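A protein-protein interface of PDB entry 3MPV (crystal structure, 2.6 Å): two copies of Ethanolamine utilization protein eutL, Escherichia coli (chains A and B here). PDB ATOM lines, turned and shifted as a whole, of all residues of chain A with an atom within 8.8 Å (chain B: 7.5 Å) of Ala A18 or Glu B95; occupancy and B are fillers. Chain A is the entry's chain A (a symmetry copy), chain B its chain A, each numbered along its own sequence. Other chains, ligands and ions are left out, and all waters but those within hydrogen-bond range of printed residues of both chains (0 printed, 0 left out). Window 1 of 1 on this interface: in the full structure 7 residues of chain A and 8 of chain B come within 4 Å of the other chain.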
ATOM      1  N   ARG A  15       6.607 -25.851   9.099  1.00  0.00           N
ATOM      2  CA  ARG A  15       6.493 -24.689   8.238  1.00  0.00           C
ATOM      3  C   ARG A  15       5.117 -24.016   8.379  1.00  0.00           C
ATOM      4  O   ARG A  15       4.072 -24.662   8.393  1.00  0.00           O
ATOM      5  CB  ARG A  15       6.731 -25.058   6.775  1.00  0.00           C
ATOM      6  CG  ARG A  15       7.662 -24.039   6.049  1.00  0.00           C
ATOM      7  CD  ARG A  15       9.100 -24.448   6.183  1.00  0.00           C
ATOM      8  NE  ARG A  15       9.243 -25.656   5.424  1.00  0.00           N
ATOM      9  CZ  ARG A  15       8.672 -26.811   5.738  1.00  0.00           C
ATOM     10  NH1 ARG A  15       7.935 -26.894   6.844  1.00  0.00           N
ATOM     11  NH2 ARG A  15       8.829 -27.880   4.934  1.00  0.00           N
ATOM     12  N   VAL A  16       5.136 -22.700   8.504  1.00  0.00           N
ATOM     13  CA  VAL A  16       3.910 -21.933   8.602  1.00  0.00           C
ATOM     14  C   VAL A  16       3.603 -21.419   7.194  1.00  0.00           C
ATOM     15  O   VAL A  16       4.531 -21.083   6.424  1.00  0.00           O
ATOM     16  CB  VAL A  16       4.049 -20.727   9.563  1.00  0.00           C
ATOM     17  CG1 VAL A  16       3.037 -19.656   9.213  1.00  0.00           C
ATOM     18  CG2 VAL A  16       3.911 -21.154  11.032  1.00  0.00           C
ATOM     19  N   ILE A  17       2.315 -21.441   6.834  1.00  0.00           N
ATOM     20  CA  ILE A  17       1.844 -20.777   5.636  1.00  0.00           C
ATOM     21  C   ILE A  17       0.976 -19.631   6.073  1.00  0.00           C
ATOM     22  O   ILE A  17      -0.215 -19.811   6.363  1.00  0.00           O
ATOM     23  CB  ILE A  17       0.961 -21.652   4.858  1.00  0.00           C
ATOM     24  CG1 ILE A  17       1.788 -22.578   3.983  1.00  0.00           C
ATOM     25  CG2 ILE A  17       0.096 -20.811   3.973  1.00  0.00           C
ATOM     26  CD1 ILE A  17       0.951 -23.595   3.225  1.00  0.00           C
ATOM     27  N   ALA A  18       1.578 -18.449   6.136  1.00  0.00           N
ATOM     28  CA  ALA A  18       0.915 -17.294   6.696  1.00  0.00           C
ATOM     29  C   ALA A  18      -0.430 -16.947   5.979  1.00  0.00           C
ATOM     30  O   ALA A  18      -1.353 -16.332   6.581  1.00  0.00           O
ATOM     31  CB  ALA A  18       1.896 -16.094   6.702  1.00  0.00           C
ATOM     32  N   SER A  19      -0.530 -17.291   4.690  1.00  0.00           N
ATOM     33  CA  SER A  19      -1.752 -16.956   3.919  1.00  0.00           C
ATOM     34  C   SER A  19      -2.069 -17.909   2.798  1.00  0.00           C
ATOM     35  O   SER A  19      -1.603 -17.720   1.701  1.00  0.00           O
ATOM     36  CB  SER A  19      -1.734 -15.519   3.381  1.00  0.00           C
ATOM     37  OG  SER A  19      -2.980 -14.833   3.713  1.00  0.00           O
ATOM     38  N   VAL A  20      -2.901 -18.907   3.123  1.00  0.00           N
ATOM     39  CA  VAL A  20      -3.186 -20.037   2.249  1.00  0.00           C
ATOM     40  C   VAL A  20      -3.890 -19.482   1.082  1.00  0.00           C
ATOM     41  O   VAL A  20      -4.721 -18.602   1.240  1.00  0.00           O
ATOM     42  CB  VAL A  20      -4.109 -21.088   2.912  1.00  0.00           C
ATOM     43  CG1 VAL A  20      -3.514 -21.577   4.227  1.00  0.00           C
ATOM     44  CG2 VAL A  20      -5.471 -20.453   3.216  1.00  0.00           C
ATOM     45  N   ASN A  21      -3.524 -19.981  -0.087  1.00  0.00           N
ATOM     46  CA  ASN A  21      -4.206 -19.663  -1.331  1.00  0.00           C
ATOM     47  C   ASN A  21      -5.728 -19.702  -1.216  1.00  0.00           C
ATOM     48  O   ASN A  21      -6.320 -20.545  -0.469  1.00  0.00           O
ATOM     49  CB  ASN A  21      -3.846 -20.693  -2.384  1.00  0.00           C
ATOM     50  CG  ASN A  21      -4.002 -20.164  -3.754  1.00  0.00           C
ATOM     51  OD1 ASN A  21      -3.824 -18.992  -3.946  1.00  0.00           O
ATOM     52  ND2 ASN A  21      -4.282 -21.025  -4.733  1.00  0.00           N
ATOM     53  N   ILE A  34     -10.305 -19.305   8.820  1.00  0.00           N
ATOM     54  CA  ILE A  34      -8.957 -19.868   8.803  1.00  0.00           C
ATOM     55  C   ILE A  34      -8.172 -19.525   7.547  1.00  0.00           C
ATOM     56  O   ILE A  34      -8.434 -20.073   6.454  1.00  0.00           O
ATOM     57  CB  ILE A  34      -9.002 -21.376   8.936  1.00  0.00           C
ATOM     58  CG1 ILE A  34      -8.937 -21.778  10.391  1.00  0.00           C
ATOM     59  CG2 ILE A  34      -7.857 -22.014   8.205  1.00  0.00           C
ATOM     60  CD1 ILE A  34      -9.418 -23.169  10.572  1.00  0.00           C
ATOM     61  N   ARG A  35      -7.206 -18.620   7.711  1.00  0.00           N
ATOM     62  CA  ARG A  35      -6.308 -18.242   6.612  1.00  0.00           C
ATOM     63  C   ARG A  35      -4.851 -18.516   6.868  1.00  0.00           C
ATOM     64  O   ARG A  35      -4.054 -18.430   5.925  1.00  0.00           O
ATOM     65  CB  ARG A  35      -6.447 -16.773   6.249  1.00  0.00           C
ATOM     66  CG  ARG A  35      -7.415 -16.542   5.081  1.00  0.00           C
ATOM     67  CD  ARG A  35      -8.885 -16.547   5.636  1.00  0.00           C
ATOM     68  NE  ARG A  35      -9.909 -16.739   4.607  1.00  0.00           N
ATOM     69  CZ  ARG A  35     -10.023 -17.831   3.850  1.00  0.00           C
ATOM     70  NH1 ARG A  35      -9.162 -18.843   3.973  1.00  0.00           N
ATOM     71  NH2 ARG A  35     -10.995 -17.902   2.949  1.00  0.00           N
ATOM     72  N   SER A  36      -4.504 -18.804   8.123  1.00  0.00           N
ATOM     73  CA  SER A  36      -3.162 -19.224   8.433  1.00  0.00           C
ATOM     74  C   SER A  36      -3.118 -20.735   8.538  1.00  0.00           C
ATOM     75  O   SER A  36      -4.132 -21.381   8.698  1.00  0.00           O
ATOM     76  CB  SER A  36      -2.657 -18.562   9.703  1.00  0.00           C
ATOM     77  OG  SER A  36      -2.048 -17.329   9.417  1.00  0.00           O
ATOM     78  N   LEU A  37      -1.931 -21.307   8.436  1.00  0.00           N
ATOM     79  CA  LEU A  37      -1.799 -22.744   8.458  1.00  0.00           C
ATOM     80  C   LEU A  37      -0.484 -23.190   9.109  1.00  0.00           C
ATOM     81  O   LEU A  37       0.579 -22.585   8.893  1.00  0.00           O
ATOM     82  CB  LEU A  37      -1.805 -23.237   7.012  1.00  0.00           C
ATOM     83  CG  LEU A  37      -2.820 -24.314   6.772  1.00  0.00           C
ATOM     84  CD1 LEU A  37      -4.119 -23.727   7.261  1.00  0.00           C
ATOM     85  CD2 LEU A  37      -2.857 -24.598   5.348  1.00  0.00           C
ATOM     86  N   GLY A  38      -0.549 -24.284   9.860  1.00  0.00           N
ATOM     87  CA  GLY A  38       0.645 -24.880  10.421  1.00  0.00           C
ATOM     88  C   GLY A  38       0.831 -26.302   9.895  1.00  0.00           C
ATOM     89  O   GLY A  38      -0.054 -27.200  10.102  1.00  0.00           O
ATOM     90  N   LEU A  39       1.972 -26.554   9.251  1.00  0.00           N
ATOM     91  CA  LEU A  39       2.338 -27.911   9.010  1.00  0.00           C
ATOM     92  C   LEU A  39       3.320 -28.472  10.022  1.00  0.00           C
ATOM     93  O   LEU A  39       4.418 -27.959  10.125  1.00  0.00           O
ATOM     94  CB  LEU A  39       2.963 -27.959   7.665  1.00  0.00           C
ATOM     95  CG  LEU A  39       2.025 -27.389   6.631  1.00  0.00           C
ATOM     96  CD1 LEU A  39       2.665 -27.648   5.322  1.00  0.00           C
ATOM     97  CD2 LEU A  39       0.665 -28.067   6.722  1.00  0.00           C
ATOM     98  N   GLY A  90      -5.685 -21.704  11.723  1.00  0.00           N
ATOM     99  CA  GLY A  90      -5.952 -20.487  12.540  1.00  0.00           C
ATOM    100  C   GLY A  90      -6.100 -19.135  11.789  1.00  0.00           C
ATOM    101  O   GLY A  90      -5.818 -18.998  10.581  1.00  0.00           O
ATOM    102  N   PRO A  91      -6.562 -18.119  12.500  1.00  0.00           N
ATOM    103  CA  PRO A  91      -6.911 -16.836  11.940  1.00  0.00           C
ATOM    104  C   PRO A  91      -5.770 -16.033  11.396  1.00  0.00           C
ATOM    105  O   PRO A  91      -5.769 -15.705  10.202  1.00  0.00           O
ATOM    106  CB  PRO A  91      -7.492 -16.080  13.141  1.00  0.00           C
ATOM    107  CG  PRO A  91      -7.084 -16.828  14.298  1.00  0.00           C
ATOM    108  CD  PRO A  91      -7.007 -18.240  13.887  1.00  0.00           C
ATOM    109  N   ASN A  92      -4.874 -15.604  12.279  1.00  0.00           N
ATOM    110  CA  ASN A  92      -3.602 -14.997  11.874  1.00  0.00           C
ATOM    111  C   ASN A  92      -2.588 -16.103  12.063  1.00  0.00           C
ATOM    112  O   ASN A  92      -2.930 -17.139  12.593  1.00  0.00           O
ATOM    113  CB  ASN A  92      -3.233 -13.884  12.835  1.00  0.00           C
ATOM    114  CG  ASN A  92      -3.553 -14.252  14.260  1.00  0.00           C
ATOM    115  OD1 ASN A  92      -4.694 -14.058  14.690  1.00  0.00           O
ATOM    116  ND2 ASN A  92      -2.587 -14.851  14.989  1.00  0.00           N
ATOM    117  N   PRO A  93      -1.336 -15.860  11.667  1.00  0.00           N
ATOM    118  CA  PRO A  93      -0.242 -16.784  11.950  1.00  0.00           C
ATOM    119  C   PRO A  93       0.121 -16.837  13.400  1.00  0.00           C
ATOM    120  O   PRO A  93       0.549 -17.873  13.879  1.00  0.00           O
ATOM    121  CB  PRO A  93       0.938 -16.200  11.144  1.00  0.00           C
ATOM    122  CG  PRO A  93       0.300 -15.453   9.995  1.00  0.00           C
ATOM    123  CD  PRO A  93      -0.993 -14.882  10.607  1.00  0.00           C
ATOM    124  N   ALA A  94      -0.029 -15.732  14.109  1.00  0.00           N
ATOM    125  CA  ALA A  94       0.535 -15.646  15.455  1.00  0.00           C
ATOM    126  C   ALA A  94      -0.154 -16.578  16.399  1.00  0.00           C
ATOM    127  O   ALA A  94       0.378 -16.837  17.501  1.00  0.00           O
ATOM    128  CB  ALA A  94       0.455 -14.209  16.001  1.00  0.00           C
ATOM    129  N   VAL A  96      -1.339 -19.620  15.090  1.00  0.00           N
ATOM    130  CA  VAL A  96      -0.924 -20.969  14.697  1.00  0.00           C
ATOM    131  C   VAL A  96       0.561 -21.244  15.071  1.00  0.00           C
ATOM    132  O   VAL A  96       1.001 -22.378  15.302  1.00  0.00           O
ATOM    133  CB  VAL A  96      -1.030 -21.210  13.231  1.00  0.00           C
ATOM    134  CG1 VAL A  96      -2.146 -20.349  12.566  1.00  0.00           C
ATOM    135  CG2 VAL A  96       0.280 -20.918  12.680  1.00  0.00           C
ATOM    136  N   ARG A  97       1.354 -20.197  15.126  1.00  0.00           N
ATOM    137  CA  ARG A  97       2.683 -20.336  15.717  1.00  0.00           C
ATOM    138  C   ARG A  97       2.573 -20.908  17.123  1.00  0.00           C
ATOM    139  O   ARG A  97       3.071 -21.994  17.374  1.00  0.00           O
ATOM    140  CB  ARG A  97       3.377 -18.995  15.748  1.00  0.00           C
ATOM    141  CG  ARG A  97       3.829 -18.584  14.382  1.00  0.00           C
ATOM    142  CD  ARG A  97       5.087 -19.360  14.067  1.00  0.00           C
ATOM    143  NE  ARG A  97       5.683 -18.991  12.794  1.00  0.00           N
ATOM    144  CZ  ARG A  97       5.703 -17.749  12.307  1.00  0.00           C
ATOM    145  NH1 ARG A  97       5.162 -16.759  13.013  1.00  0.00           N
ATOM    146  NH2 ARG A  97       6.288 -17.500  11.124  1.00  0.00           N
ATOM    147  N   SER B  36      -1.658  -2.339  11.323  1.00  0.00           N
ATOM    148  CA  SER B  36      -0.249  -2.632  11.376  1.00  0.00           C
ATOM    149  C   SER B  36       0.432  -2.065  10.147  1.00  0.00           C
ATOM    150  O   SER B  36      -0.207  -1.766   9.160  1.00  0.00           O
ATOM    151  CB  SER B  36      -0.002  -4.125  11.511  1.00  0.00           C
ATOM    152  OG  SER B  36       0.016  -4.509  12.862  1.00  0.00           O
ATOM    153  N   ALA B  55       4.746 -10.173  -1.860  1.00  0.00           N
ATOM    154  CA  ALA B  55       4.443 -10.436  -0.471  1.00  0.00           C
ATOM    155  C   ALA B  55       2.954 -10.153  -0.270  1.00  0.00           C
ATOM    156  O   ALA B  55       2.301 -10.687   0.680  1.00  0.00           O
ATOM    157  CB  ALA B  55       5.325  -9.587   0.463  1.00  0.00           C
ATOM    158  N   LYS B  57       1.066 -11.812  -1.580  1.00  0.00           N
ATOM    159  CA  LYS B  57       0.456 -13.129  -1.827  1.00  0.00           C
ATOM    160  C   LYS B  57       0.782 -14.120  -0.751  1.00  0.00           C
ATOM    161  O   LYS B  57       0.397 -15.309  -0.784  1.00  0.00           O
ATOM    162  CB  LYS B  57       0.931 -13.730  -3.144  1.00  0.00           C
ATOM    163  CG  LYS B  57       1.184 -12.704  -4.213  1.00  0.00           C
ATOM    164  CD  LYS B  57       1.235 -13.344  -5.597  1.00  0.00           C
ATOM    165  CE  LYS B  57       2.425 -14.289  -5.645  1.00  0.00           C
ATOM    166  NZ  LYS B  57       2.849 -14.562  -7.035  1.00  0.00           N
ATOM    167  N   GLN B  58       1.519 -13.689   0.239  1.00  0.00           N
ATOM    168  CA  GLN B  58       2.051 -14.670   1.136  1.00  0.00           C
ATOM    169  C   GLN B  58       1.652 -14.234   2.487  1.00  0.00           C
ATOM    170  O   GLN B  58       1.631 -15.023   3.433  1.00  0.00           O
ATOM    171  CB  GLN B  58       3.549 -14.676   0.985  1.00  0.00           C
ATOM    172  CG  GLN B  58       3.947 -14.976  -0.467  1.00  0.00           C
ATOM    173  CD  GLN B  58       3.999 -16.434  -0.546  1.00  0.00           C
ATOM    174  OE1 GLN B  58       3.911 -17.069   0.495  1.00  0.00           O
ATOM    175  NE2 GLN B  58       4.115 -17.003  -1.721  1.00  0.00           N
ATOM    176  N   ALA B  59       1.332 -12.964   2.609  1.00  0.00           N
ATOM    177  CA  ALA B  59       0.693 -12.531   3.817  1.00  0.00           C
ATOM    178  C   ALA B  59      -0.413 -11.646   3.343  1.00  0.00           C
ATOM    179  O   ALA B  59      -0.273 -10.977   2.304  1.00  0.00           O
ATOM    180  CB  ALA B  59       1.653 -11.747   4.734  1.00  0.00           C
ATOM    181  N   MET B  60      -1.499 -11.607   4.118  1.00  0.00           N
ATOM    182  CA  MET B  60      -2.632 -10.751   3.802  1.00  0.00           C
ATOM    183  C   MET B  60      -2.220  -9.346   4.003  1.00  0.00           C
ATOM    184  O   MET B  60      -2.392  -8.792   5.089  1.00  0.00           O
ATOM    185  CB  MET B  60      -3.761 -11.068   4.758  1.00  0.00           C
ATOM    186  CG  MET B  60      -5.155 -10.990   4.150  1.00  0.00           C
ATOM    187  SD  MET B  60      -6.102 -12.189   5.157  1.00  0.00           S
ATOM    188  CE  MET B  60      -6.098 -13.597   4.054  1.00  0.00           C
ATOM    189  N   VAL B  61      -1.628  -8.745   2.990  1.00  0.00           N
ATOM    190  CA  VAL B  61      -1.061  -7.426   3.239  1.00  0.00           C
ATOM    191  C   VAL B  61      -1.366  -6.708   2.004  1.00  0.00           C
ATOM    192  O   VAL B  61      -1.830  -7.302   1.066  1.00  0.00           O
ATOM    193  CB  VAL B  61       0.494  -7.466   3.504  1.00  0.00           C
ATOM    194  CG1 VAL B  61       0.846  -8.578   4.506  1.00  0.00           C
ATOM    195  CG2 VAL B  61       1.253  -7.692   2.252  1.00  0.00           C
ATOM    196  N   GLU B  62      -1.091  -5.418   1.996  1.00  0.00           N
ATOM    197  CA  GLU B  62      -1.133  -4.687   0.750  1.00  0.00           C
ATOM    198  C   GLU B  62      -0.167  -3.509   0.790  1.00  0.00           C
ATOM    199  O   GLU B  62       0.205  -3.029   1.852  1.00  0.00           O
ATOM    200  CB  GLU B  62      -2.573  -4.243   0.471  1.00  0.00           C
ATOM    201  CG  GLU B  62      -2.698  -3.643  -0.896  1.00  0.00           C
ATOM    202  CD  GLU B  62      -2.276  -4.584  -1.982  1.00  0.00           C
ATOM    203  OE1 GLU B  62      -2.409  -5.829  -1.705  1.00  0.00           O
ATOM    204  OE2 GLU B  62      -1.844  -4.087  -3.083  1.00  0.00           O
ATOM    205  N   LEU B  88       4.068  -1.546   3.827  1.00  0.00           N
ATOM    206  CA  LEU B  88       3.089  -2.625   3.646  1.00  0.00           C
ATOM    207  C   LEU B  88       2.011  -2.557   4.717  1.00  0.00           C
ATOM    208  O   LEU B  88       2.365  -2.621   5.919  1.00  0.00           O
ATOM    209  CB  LEU B  88       3.769  -3.944   3.858  1.00  0.00           C
ATOM    210  CG  LEU B  88       4.404  -4.689   2.708  1.00  0.00           C
ATOM    211  CD1 LEU B  88       5.257  -5.722   3.392  1.00  0.00           C
ATOM    212  CD2 LEU B  88       3.411  -5.356   1.798  1.00  0.00           C
ATOM    213  N   GLY B  89       0.729  -2.459   4.317  1.00  0.00           N
ATOM    214  CA  GLY B  89      -0.386  -2.445   5.289  1.00  0.00           C
ATOM    215  C   GLY B  89      -1.011  -3.807   5.596  1.00  0.00           C
ATOM    216  O   GLY B  89      -1.225  -4.595   4.666  1.00  0.00           O
ATOM    217  N   GLY B  90      -1.316  -4.060   6.886  1.00  0.00           N
ATOM    218  CA  GLY B  90      -2.026  -5.279   7.366  1.00  0.00           C
ATOM    219  C   GLY B  90      -2.769  -5.189   8.727  1.00  0.00           C
ATOM    220  O   GLY B  90      -2.635  -4.226   9.508  1.00  0.00           O
ATOM    221  N   PRO B  91      -3.576  -6.196   9.020  1.00  0.00           N
ATOM    222  CA  PRO B  91      -4.461  -6.215  10.160  1.00  0.00           C
ATOM    223  C   PRO B  91      -3.794  -6.262  11.499  1.00  0.00           C
ATOM    224  O   PRO B  91      -3.995  -5.352  12.314  1.00  0.00           O
ATOM    225  CB  PRO B  91      -5.241  -7.522   9.972  1.00  0.00           C
ATOM    226  CG  PRO B  91      -4.495  -8.276   9.003  1.00  0.00           C
ATOM    227  CD  PRO B  91      -3.854  -7.302   8.104  1.00  0.00           C
ATOM    228  N   ASN B  92      -3.116  -7.369  11.784  1.00  0.00           N
ATOM    229  CA  ASN B  92      -2.241  -7.474  12.955  1.00  0.00           C
ATOM    230  C   ASN B  92      -0.848  -7.308  12.392  1.00  0.00           C
ATOM    231  O   ASN B  92      -0.694  -7.267  11.189  1.00  0.00           O
ATOM    232  CB  ASN B  92      -2.323  -8.871  13.537  1.00  0.00           C
ATOM    233  CG  ASN B  92      -2.382  -9.920  12.458  1.00  0.00           C
ATOM    234  OD1 ASN B  92      -3.474 -10.212  11.961  1.00  0.00           O
ATOM    235  ND2 ASN B  92      -1.217 -10.447  12.027  1.00  0.00           N
ATOM    236  N   PRO B  93       0.163  -7.256  13.264  1.00  0.00           N
ATOM    237  CA  PRO B  93       1.558  -7.266  12.832  1.00  0.00           C
ATOM    238  C   PRO B  93       1.986  -8.580  12.260  1.00  0.00           C
ATOM    239  O   PRO B  93       2.835  -8.610  11.386  1.00  0.00           O
ATOM    240  CB  PRO B  93       2.338  -6.991  14.136  1.00  0.00           C
ATOM    241  CG  PRO B  93       1.385  -6.207  15.008  1.00  0.00           C
ATOM    242  CD  PRO B  93       0.006  -6.803  14.667  1.00  0.00           C
ATOM    243  N   ALA B  94       1.424  -9.670  12.747  1.00  0.00           N
ATOM    244  CA  ALA B  94       1.970 -10.985  12.414  1.00  0.00           C
ATOM    245  C   ALA B  94       1.788 -11.303  10.965  1.00  0.00           C
ATOM    246  O   ALA B  94       2.439 -12.245  10.458  1.00  0.00           O
ATOM    247  CB  ALA B  94       1.323 -12.091  13.268  1.00  0.00           C
ATOM    248  N   GLU B  95       0.862 -10.582  10.322  1.00  0.00           N
ATOM    249  CA  GLU B  95       0.645 -10.696   8.881  1.00  0.00           C
ATOM    250  C   GLU B  95       1.485  -9.727   8.091  1.00  0.00           C
ATOM    251  O   GLU B  95       1.718  -9.979   6.905  1.00  0.00           O
ATOM    252  CB  GLU B  95      -0.810 -10.444   8.487  1.00  0.00           C
ATOM    253  CG  GLU B  95      -1.653 -11.716   8.376  1.00  0.00           C
ATOM    254  CD  GLU B  95      -1.030 -12.784   7.501  1.00  0.00           C
ATOM    255  OE1 GLU B  95      -1.504 -13.954   7.527  1.00  0.00           O
ATOM    256  OE2 GLU B  95      -0.060 -12.456   6.783  1.00  0.00           O
ATOM    257  N   VAL B  96       1.924  -8.621   8.692  1.00  0.00           N
ATOM    258  CA  VAL B  96       2.846  -7.742   7.970  1.00  0.00           C
ATOM    259  C   VAL B  96       4.327  -8.178   8.166  1.00  0.00           C
ATOM    260  O   VAL B  96       5.215  -7.948   7.333  1.00  0.00           O
ATOM    261  CB  VAL B  96       2.773  -6.323   8.418  1.00  0.00           C
ATOM    262  CG1 VAL B  96       1.365  -5.945   8.967  1.00  0.00           C
ATOM    263  CG2 VAL B  96       3.807  -6.165   9.423  1.00  0.00           C
ATOM    264  N   ARG B  97       4.608  -8.810   9.283  1.00  0.00           N
ATOM    265  CA  ARG B  97       5.902  -9.475   9.424  1.00  0.00           C
ATOM    266  C   ARG B  97       6.118 -10.448   8.274  1.00  0.00           C
ATOM    267  O   ARG B  97       7.039 -10.267   7.495  1.00  0.00           O
ATOM    268  CB  ARG B  97       5.968 -10.200  10.747  1.00  0.00           C
ATOM    269  CG  ARG B  97       6.132  -9.243  11.885  1.00  0.00           C
ATOM    270  CD  ARG B  97       7.581  -8.814  11.914  1.00  0.00           C
ATOM    271  NE  ARG B  97       7.897  -7.942  13.033  1.00  0.00           N
ATOM    272  CZ  ARG B  97       7.367  -8.063  14.252  1.00  0.00           C
ATOM    273  NH1 ARG B  97       6.499  -9.041  14.494  1.00  0.00           N
ATOM    274  NH2 ARG B  97       7.729  -7.216  15.229  1.00  0.00           N
ATOM    275  N   ALA B  98       5.292 -11.493   8.187  1.00  0.00           N
ATOM    276  CA  ALA B  98       5.490 -12.526   7.191  1.00  0.00           C
ATOM    277  C   ALA B  98       5.596 -11.896   5.854  1.00  0.00           C
ATOM    278  O   ALA B  98       6.172 -12.458   4.930  1.00  0.00           O
ATOM    279  CB  ALA B  98       4.316 -13.451   7.191  1.00  0.00           C
ATOM    280  N   GLY B  99       4.947 -10.742   5.739  1.00  0.00           N
ATOM    281  CA  GLY B  99       4.947  -9.995   4.509  1.00  0.00           C
ATOM    282  C   GLY B  99       6.303  -9.378   4.242  1.00  0.00           C
ATOM    283  O   GLY B  99       6.822  -9.475   3.155  1.00  0.00           O
ATOM    284  N   LEU B 100       6.822  -8.641   5.206  1.00  0.00           N
ATOM    285  CA  LEU B 100       8.157  -8.075   5.082  1.00  0.00           C
ATOM    286  C   LEU B 100       9.224  -9.139   4.879  1.00  0.00           C
ATOM    287  O   LEU B 100      10.011  -9.049   3.957  1.00  0.00           O
ATOM    288  CB  LEU B 100       8.495  -7.377   6.353  1.00  0.00           C
ATOM    289  CG  LEU B 100       7.921  -6.019   6.688  1.00  0.00           C
ATOM    290  CD1 LEU B 100       8.591  -5.635   8.029  1.00  0.00           C
ATOM    291  CD2 LEU B 100       8.201  -5.064   5.657  1.00  0.00           C
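O of Gln B58 sits at hydrogen-bond distance from N of Ser A19 (3.4 Å).
The backbone carbonyl oxygen (O) of Ala A18 sits close to the side-chain carboxylate (OE1) of Glu B95, 2.6 Å away.
O of Asn B92 sits close to OG of Ser B36 (3.3 Å).
OE2 of Glu B95 lies within hydrogen-bond range of N of Met B60 (3.1 Å).
O of Ala A18 is in hydrogen-bond range of OG of Ser A36 (3.1 Å).
N of Ser A36 is in hydrogen-bond range of O of Gly A90, at 2.8 Å.
O of Asn A92 sits close to OG of Ser A36 (3.3 Å).
N of Ala A94 sits close to ND2 of Asn A92 (2.8 Å).
Ala B98 touches Ala A18.
Ser A19 touches Lys B57 (O to O, 3.999 Å).
CA of Ala B59 touches CB of Ser A19, at 3.9 Å.
Ser A19 touches Met B60.
Arg A35 touches Met B60.
Ser A36 touches Glu B95 (OG to OE1, 3.9 Å).
OD1 of Asn B92 touches CB of Asn A92, at 3.8 Å.
CG of Pro A93 touches O of Ala B94, 3.9 Å away.
Glu B95 touches Pro A93.
CB of Ala B94 touches CB of Ala A94 (3.6 Å).
Ala A18 touches three residues of chain B.
Glu B95 touches three residues of chain A.
Ala B59 touches just one residue of chain A: Ser A19 (3.9 Å).
Of chain A, only Pro A93 and Ala A94 come within 4 Å of Ala B94.
No residue of chain A comes within 4 Å of Val B96.
Of the printed residues of chain B, Asn A92 touches Asn B92.
Of the printed residues of chain A, Ala B98 touches Ala A18.
Of the printed residues of chain A, Met B60 touches Ser A19 and Arg A35.
Of the printed residues of chain A, Asn B92 touches Asn A92 (3.8 Å).
Arg B97 touches none of the printed residues of chain A.
The nearest residue of chain A that does not touch Glu B95 is Ser A19 (4.2 Å).
Of the 20 printed residues of chain A, 7 touch a printed residue of chain B.
Hydrophobic or aromatic side chains of chain A that line the printed part of chain B: Ala A18, Pro A93 and Ala A94.
Hydrophobic or aromatic side chains of chain B within 4 Å of the printed part of chain A: Met B60, Ala B94 and Ala B98.
Among the printed residues, no Asp or Glu carboxylate lies within 4 Å of a Lys or Arg side-chain nitrogen of the other chain.
Asn B92 touches its own counterpart, Asn A92.
Pro A93 touches Ala B94, but with the chains exchanged Ala A94 does not touch Pro B93 (6.9 Å).
Ala B94 touches its own counterpart, Ala A94.
Of the 13 pairs that touch across the chains among the printed residues, 2 have their exchanged pair printed and touching as well.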
